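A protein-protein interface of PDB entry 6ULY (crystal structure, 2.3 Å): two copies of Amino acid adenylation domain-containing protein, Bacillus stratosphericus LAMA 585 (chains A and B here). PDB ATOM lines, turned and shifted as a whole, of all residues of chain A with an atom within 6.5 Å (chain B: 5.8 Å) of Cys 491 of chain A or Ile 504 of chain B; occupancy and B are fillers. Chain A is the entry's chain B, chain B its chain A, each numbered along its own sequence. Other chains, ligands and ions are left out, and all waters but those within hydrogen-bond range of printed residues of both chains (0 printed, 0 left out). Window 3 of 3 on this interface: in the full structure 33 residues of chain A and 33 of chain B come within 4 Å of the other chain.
SG of Cys 491 of chain B is disulfide-bonded to SG of Cys 491 of chain A, 2.0 Å away. The backbone NH of Ser 492 of chain A lies within hydrogen-bond range of the side-chain sulfur of Cys 491 of chain B (3.0 Å). The backbone carbonyl oxygen (O) of Ser 492 of chain A sits close to the backbone carbonyl oxygen (O) of Ala 490 of chain B.
Cys 491 of chain A touches two residues of chain B. Ile 504 of chain B touches two residues of chain A. Printed residues of chain A within 4 Å of Ile 540 of chain B: Ile 504. Of the printed residues of chain B, Ile 540 of chain A touches Val 542 (3.6 Å). Of the printed residues of chain B, Ile 504 of chain A touches Ile 504 (3.9 Å) and Ile 540 (3.9 Å). Phe 487 of chain B touches none of the printed residues of chain A. The nearest residue of chain B that does not touch Cys 491 of chain A is Ser 492 of chain B (4.3 Å). The nearest residue of chain A that does not touch Ile 504 of chain B is Ile 540 of chain A (4.1 Å).
Ala 490 of chain A touches Ser 492 of chain B, and with the chains exchanged Ser 492 of chain A touches Ala 490 of chain B. Cys 491 of chain B touches its own counterpart, Cys 491 of chain A. Cys 491 of chain A touches Ile 504 of chain B, but with the chains exchanged Ile 504 of chain A does not touch Cys 491 of chain B (5.3 Å). Ile 504 of chain A touches Ile 540 of chain B, but with the chains exchanged Ile 540 of chain A does not touch Ile 504 of chain B (4.1 Å). Positions printed for both chains: 489, 490, 491, 492, 503, 504 and 540. Of the 8 pairs that touch across the chains among the printed residues, 4 have their exchanged pair printed and touching as well.
Among the printed residues, pairs that only touch across the chains: Ile 540 of chain A with Val 542 of chain B (3.6 Å), Cys 491 of chain A with Ile 504 of chain B (3.7 Å), Ala 490 of chain A with Ser 492 of chain B (3.7 Å), Ile 504 of chain A with Ile 540 of chain B (3.9 Å) and Ile 504 of chain A with Ile 504 of chain B (3.9 Å).
N of Cys 491 of chain B is in hydrogen-bond range of O of Glu 502 of chain B (2.8 Å). The backbone carbonyl oxygen of Leu 503 of chain B is in hydrogen-bond range of the backbone NH of Ile 540 of chain B (3.4 Å). N of Leu 505 of chain B sits at hydrogen-bond distance from O of Ile 540 of chain B, at 2.9 Å. The backbone carbonyl oxygen (O) of Leu 505 of chain B lies within hydrogen-bond range of the backbone NH (N) of Val 542 of chain B (3.0 Å). The backbone NH (N) of Ala 489 of chain A sits at hydrogen-bond distance from the backbone carbonyl oxygen (O) of Ile 504 of chain A, at 3.1 Å. The backbone carbonyl oxygen (O) of Leu 503 of chain A sits at hydrogen-bond distance from the backbone NH (N) of Ile 540 of chain A.
Hydrophobic or aromatic side chains of chain B that line the printed part of chain A: Ile 504, Ile 540 and Val 542. Along chain A the printed residues that touch a printed residue of chain B span positions 490 to 540. Among the printed residues, 8 pairs touch across the chains.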
ATOM      1  N   ILE A 461     -11.604 -28.105  30.777  1.00  0.00           N
ATOM      2  CA  ILE A 461     -11.373 -28.308  29.317  1.00  0.00           C
ATOM      3  C   ILE A 461     -12.728 -28.516  28.635  1.00  0.00           C
ATOM      4  O   ILE A 461     -13.464 -29.427  29.059  1.00  0.00           O
ATOM      5  CB  ILE A 461     -10.433 -29.508  29.094  1.00  0.00           C
ATOM      6  CG1 ILE A 461      -9.213 -29.445  30.016  1.00  0.00           C
ATOM      7  CG2 ILE A 461     -10.031 -29.619  27.632  1.00  0.00           C
ATOM      8  CD1 ILE A 461      -9.391 -30.182  31.322  1.00  0.00           C
ATOM      9  N   ALA A 489      -3.560 -29.207  31.044  1.00  0.00           N
ATOM     10  CA  ALA A 489      -3.943 -27.821  31.229  1.00  0.00           C
ATOM     11  C   ALA A 489      -4.579 -27.379  29.905  1.00  0.00           C
ATOM     12  O   ALA A 489      -3.901 -27.478  28.850  1.00  0.00           O
ATOM     13  CB  ALA A 489      -2.733 -27.011  31.574  1.00  0.00           C
ATOM     14  N   ALA A 490      -5.831 -26.899  29.943  1.00  0.00           N
ATOM     15  CA  ALA A 490      -6.635 -26.487  28.767  1.00  0.00           C
ATOM     16  C   ALA A 490      -5.915 -25.402  27.949  1.00  0.00           C
ATOM     17  O   ALA A 490      -5.250 -24.539  28.559  1.00  0.00           O
ATOM     18  CB  ALA A 490      -7.990 -26.006  29.227  1.00  0.00           C
ATOM     19  N   CYS A 491      -6.083 -25.418  26.619  1.00  0.00           N
ATOM     20  CA  CYS A 491      -5.480 -24.453  25.662  1.00  0.00           C
ATOM     21  C   CYS A 491      -6.589 -23.861  24.784  1.00  0.00           C
ATOM     22  O   CYS A 491      -7.516 -24.616  24.431  1.00  0.00           O
ATOM     23  CB  CYS A 491      -4.448 -25.131  24.770  1.00  0.00           C
ATOM     24  SG  CYS A 491      -2.951 -24.145  24.502  1.00  0.00           S
ATOM     25  N   SER A 492      -6.499 -22.572  24.440  1.00  0.00           N
ATOM     26  CA  SER A 492      -7.481 -21.861  23.582  1.00  0.00           C
ATOM     27  C   SER A 492      -6.739 -21.246  22.384  1.00  0.00           C
ATOM     28  O   SER A 492      -5.769 -20.504  22.632  1.00  0.00           O
ATOM     29  CB  SER A 492      -8.222 -20.812  24.369  1.00  0.00           C
ATOM     30  OG  SER A 492      -8.946 -21.404  25.438  1.00  0.00           O
ATOM     31  N   VAL A 493      -7.163 -21.524  21.141  1.00  0.00           N
ATOM     32  CA  VAL A 493      -6.531 -21.004  19.906  1.00  0.00           C
ATOM     33  C   VAL A 493      -7.263 -19.736  19.450  1.00  0.00           C
ATOM     34  O   VAL A 493      -8.399 -19.535  19.924  1.00  0.00           O
ATOM     35  CB  VAL A 493      -6.545 -22.043  18.770  1.00  0.00           C
ATOM     36  CG1 VAL A 493      -6.003 -21.437  17.485  1.00  0.00           C
ATOM     37  CG2 VAL A 493      -5.746 -23.275  19.165  1.00  0.00           C
ATOM     38  N   LEU A 503      -5.527 -29.174  24.235  1.00  0.00           N
ATOM     39  CA  LEU A 503      -5.392 -30.019  25.450  1.00  0.00           C
ATOM     40  C   LEU A 503      -3.892 -30.327  25.657  1.00  0.00           C
ATOM     41  O   LEU A 503      -3.402 -31.255  25.086  1.00  0.00           O
ATOM     42  CB  LEU A 503      -6.276 -31.256  25.251  1.00  0.00           C
ATOM     43  CG  LEU A 503      -6.391 -32.197  26.427  1.00  0.00           C
ATOM     44  CD1 LEU A 503      -7.734 -32.832  26.482  1.00  0.00           C
ATOM     45  CD2 LEU A 503      -5.335 -33.272  26.340  1.00  0.00           C
ATOM     46  N   ILE A 504      -3.179 -29.479  26.400  1.00  0.00           N
ATOM     47  CA  ILE A 504      -1.720 -29.654  26.663  1.00  0.00           C
ATOM     48  C   ILE A 504      -1.549 -30.731  27.733  1.00  0.00           C
ATOM     49  O   ILE A 504      -1.652 -30.379  28.923  1.00  0.00           O
ATOM     50  CB  ILE A 504      -1.072 -28.330  27.112  1.00  0.00           C
ATOM     51  CG1 ILE A 504      -1.101 -27.271  26.010  1.00  0.00           C
ATOM     52  CG2 ILE A 504       0.340 -28.570  27.622  1.00  0.00           C
ATOM     53  CD1 ILE A 504      -0.677 -25.905  26.483  1.00  0.00           C
ATOM     54  N   ILE A 540      -2.107 -32.315  22.550  1.00  0.00           N
ATOM     55  CA  ILE A 540      -0.661 -31.953  22.511  1.00  0.00           C
ATOM     56  C   ILE A 540       0.051 -32.760  23.600  1.00  0.00           C
ATOM     57  O   ILE A 540      -0.175 -32.463  24.789  1.00  0.00           O
ATOM     58  CB  ILE A 540      -0.467 -30.436  22.702  1.00  0.00           C
ATOM     59  CG1 ILE A 540      -0.897 -29.646  21.463  1.00  0.00           C
ATOM     60  CG2 ILE A 540       0.967 -30.121  23.100  1.00  0.00           C
ATOM     61  CD1 ILE A 540      -1.508 -28.300  21.774  1.00  0.00           C
ATOM     62  N   PHE B 487       4.524 -22.437  13.079  1.00  0.00           N
ATOM     63  CA  PHE B 487       3.237 -21.722  13.247  1.00  0.00           C
ATOM     64  C   PHE B 487       3.009 -21.555  14.747  1.00  0.00           C
ATOM     65  O   PHE B 487       2.933 -22.562  15.475  1.00  0.00           O
ATOM     66  CB  PHE B 487       2.104 -22.472  12.536  1.00  0.00           C
ATOM     67  CG  PHE B 487       0.741 -21.814  12.579  1.00  0.00           C
ATOM     68  CD1 PHE B 487       0.395 -20.804  11.688  1.00  0.00           C
ATOM     69  CD2 PHE B 487      -0.212 -22.224  13.504  1.00  0.00           C
ATOM     70  CE1 PHE B 487      -0.860 -20.210  11.731  1.00  0.00           C
ATOM     71  CE2 PHE B 487      -1.466 -21.629  13.546  1.00  0.00           C
ATOM     72  CZ  PHE B 487      -1.788 -20.623  12.661  1.00  0.00           C
ATOM     73  N   VAL B 488       2.925 -20.308  15.196  1.00  0.00           N
ATOM     74  CA  VAL B 488       2.684 -19.971  16.629  1.00  0.00           C
ATOM     75  C   VAL B 488       1.217 -19.523  16.807  1.00  0.00           C
ATOM     76  O   VAL B 488       0.725 -18.729  15.995  1.00  0.00           O
ATOM     77  CB  VAL B 488       3.697 -18.914  17.114  1.00  0.00           C
ATOM     78  CG1 VAL B 488       3.569 -17.598  16.366  1.00  0.00           C
ATOM     79  CG2 VAL B 488       3.598 -18.698  18.622  1.00  0.00           C
ATOM     80  N   ALA B 489       0.520 -20.066  17.802  1.00  0.00           N
ATOM     81  CA  ALA B 489      -0.748 -19.509  18.325  1.00  0.00           C
ATOM     82  C   ALA B 489      -0.529 -19.220  19.808  1.00  0.00           C
ATOM     83  O   ALA B 489       0.060 -20.075  20.488  1.00  0.00           O
ATOM     84  CB  ALA B 489      -1.896 -20.466  18.090  1.00  0.00           C
ATOM     85  N   ALA B 490      -0.927 -18.046  20.288  1.00  0.00           N
ATOM     86  CA  ALA B 490      -0.920 -17.748  21.737  1.00  0.00           C
ATOM     87  C   ALA B 490      -1.928 -18.696  22.391  1.00  0.00           C
ATOM     88  O   ALA B 490      -2.704 -19.351  21.639  1.00  0.00           O
ATOM     89  CB  ALA B 490      -1.229 -16.298  22.002  1.00  0.00           C
ATOM     90  N   CYS B 491      -1.927 -18.837  23.722  1.00  0.00           N
ATOM     91  CA  CYS B 491      -2.847 -19.770  24.432  1.00  0.00           C
ATOM     92  C   CYS B 491      -2.993 -19.433  25.923  1.00  0.00           C
ATOM     93  O   CYS B 491      -2.047 -19.723  26.679  1.00  0.00           O
ATOM     94  CB  CYS B 491      -2.343 -21.206  24.333  1.00  0.00           C
ATOM     95  SG  CYS B 491      -3.596 -22.377  23.749  1.00  0.00           S
ATOM     96  N   SER B 492      -4.136 -18.885  26.353  1.00  0.00           N
ATOM     97  CA  SER B 492      -4.409 -18.581  27.775  1.00  0.00           C
ATOM     98  C   SER B 492      -4.462 -19.914  28.539  1.00  0.00           C
ATOM     99  O   SER B 492      -5.051 -20.867  27.992  1.00  0.00           O
ATOM    100  CB  SER B 492      -5.718 -17.806  27.942  1.00  0.00           C
ATOM    101  OG  SER B 492      -6.824 -18.569  27.492  1.00  0.00           O
ATOM    102  N   GLU B 502       0.985 -18.643  27.587  1.00  0.00           N
ATOM    103  CA  GLU B 502       1.963 -19.445  26.809  1.00  0.00           C
ATOM    104  C   GLU B 502       1.630 -19.473  25.319  1.00  0.00           C
ATOM    105  O   GLU B 502       0.438 -19.533  24.956  1.00  0.00           O
ATOM    106  CB  GLU B 502       2.004 -20.878  27.348  1.00  0.00           C
ATOM    107  CG  GLU B 502       2.492 -20.978  28.782  1.00  0.00           C
ATOM    108  CD  GLU B 502       3.964 -21.322  28.926  1.00  0.00           C
ATOM    109  OE1 GLU B 502       4.576 -20.892  29.923  1.00  0.00           O
ATOM    110  OE2 GLU B 502       4.496 -22.019  28.039  1.00  0.00           O
ATOM    111  N   LEU B 503       2.691 -19.431  24.512  1.00  0.00           N
ATOM    112  CA  LEU B 503       2.677 -19.537  23.027  1.00  0.00           C
ATOM    113  C   LEU B 503       3.061 -20.976  22.647  1.00  0.00           C
ATOM    114  O   LEU B 503       4.119 -21.454  23.104  1.00  0.00           O
ATOM    115  CB  LEU B 503       3.631 -18.497  22.423  1.00  0.00           C
ATOM    116  CG  LEU B 503       5.126 -18.707  22.676  1.00  0.00           C
ATOM    117  CD1 LEU B 503       5.793 -19.439  21.515  1.00  0.00           C
ATOM    118  CD2 LEU B 503       5.825 -17.380  22.928  1.00  0.00           C
ATOM    119  N   ILE B 504       2.184 -21.690  21.895  1.00  0.00           N
ATOM    120  CA  ILE B 504       2.376 -23.081  21.401  1.00  0.00           C
ATOM    121  C   ILE B 504       2.992 -22.955  19.994  1.00  0.00           C
ATOM    122  O   ILE B 504       2.312 -22.389  19.117  1.00  0.00           O
ATOM    123  CB  ILE B 504       1.036 -23.841  21.365  1.00  0.00           C
ATOM    124  CG1 ILE B 504       0.037 -23.279  22.380  1.00  0.00           C
ATOM    125  CG2 ILE B 504       1.257 -25.333  21.559  1.00  0.00           C
ATOM    126  CD1 ILE B 504       0.541 -23.284  23.805  1.00  0.00           C
ATOM    127  N   LEU B 505       4.214 -23.452  19.782  1.00  0.00           N
ATOM    128  CA  LEU B 505       4.992 -23.364  18.521  1.00  0.00           C
ATOM    129  C   LEU B 505       4.883 -24.710  17.784  1.00  0.00           C
ATOM    130  O   LEU B 505       5.611 -25.659  18.137  1.00  0.00           O
ATOM    131  CB  LEU B 505       6.437 -22.982  18.891  1.00  0.00           C
ATOM    132  CG  LEU B 505       7.277 -22.279  17.821  1.00  0.00           C
ATOM    133  CD1 LEU B 505       7.715 -23.247  16.737  1.00  0.00           C
ATOM    134  CD2 LEU B 505       6.540 -21.103  17.215  1.00  0.00           C
ATOM    135  N   PHE B 506       3.983 -24.805  16.802  1.00  0.00           N
ATOM    136  CA  PHE B 506       3.933 -25.953  15.859  1.00  0.00           C
ATOM    137  C   PHE B 506       5.105 -25.850  14.887  1.00  0.00           C
ATOM    138  O   PHE B 506       5.474 -24.739  14.468  1.00  0.00           O
ATOM    139  CB  PHE B 506       2.625 -25.993  15.069  1.00  0.00           C
ATOM    140  CG  PHE B 506       1.405 -26.216  15.924  1.00  0.00           C
ATOM    141  CD1 PHE B 506       1.079 -27.488  16.374  1.00  0.00           C
ATOM    142  CD2 PHE B 506       0.599 -25.150  16.303  1.00  0.00           C
ATOM    143  CE1 PHE B 506      -0.040 -27.689  17.172  1.00  0.00           C
ATOM    144  CE2 PHE B 506      -0.517 -25.351  17.103  1.00  0.00           C
ATOM    145  CZ  PHE B 506      -0.838 -26.622  17.532  1.00  0.00           C
ATOM    146  N   ARG B 538       7.799 -20.672  28.730  1.00  0.00           N
ATOM    147  CA  ARG B 538       6.710 -19.978  27.988  1.00  0.00           C
ATOM    148  C   ARG B 538       6.537 -20.538  26.569  1.00  0.00           C
ATOM    149  O   ARG B 538       5.541 -20.160  25.921  1.00  0.00           O
ATOM    150  CB  ARG B 538       6.992 -18.473  27.932  1.00  0.00           C
ATOM    151  CG  ARG B 538       6.349 -17.680  29.061  1.00  0.00           C
ATOM    152  CD  ARG B 538       7.168 -16.465  29.457  1.00  0.00           C
ATOM    153  NE  ARG B 538       7.399 -16.398  30.893  1.00  0.00           N
ATOM    154  CZ  ARG B 538       8.255 -15.567  31.478  1.00  0.00           C
ATOM    155  NH1 ARG B 538       8.965 -14.726  30.748  1.00  0.00           N
ATOM    156  NH2 ARG B 538       8.395 -15.580  32.792  1.00  0.00           N
ATOM    157  N   ILE B 540       6.222 -23.946  24.044  1.00  0.00           N
ATOM    158  CA  ILE B 540       5.931 -25.408  23.972  1.00  0.00           C
ATOM    159  C   ILE B 540       6.138 -25.840  22.516  1.00  0.00           C
ATOM    160  O   ILE B 540       5.416 -25.311  21.648  1.00  0.00           O
ATOM    161  CB  ILE B 540       4.499 -25.708  24.458  1.00  0.00           C
ATOM    162  CG1 ILE B 540       4.425 -25.805  25.984  1.00  0.00           C
ATOM    163  CG2 ILE B 540       3.954 -26.959  23.787  1.00  0.00           C
ATOM    164  CD1 ILE B 540       3.168 -25.209  26.575  1.00  0.00           C
ATOM    165  N   VAL B 542       5.574 -28.326  19.440  1.00  0.00           N
ATOM    166  CA  VAL B 542       4.705 -29.440  18.965  1.00  0.00           C
ATOM    167  C   VAL B 542       5.077 -29.782  17.519  1.00  0.00           C
ATOM    168  O   VAL B 542       4.966 -28.897  16.649  1.00  0.00           O
ATOM    169  CB  VAL B 542       3.213 -29.075  19.084  1.00  0.00           C
ATOM    170  CG1 VAL B 542       2.315 -30.231  18.671  1.00  0.00           C
ATOM    171  CG2 VAL B 542       2.861 -28.597  20.484  1.00  0.00           C
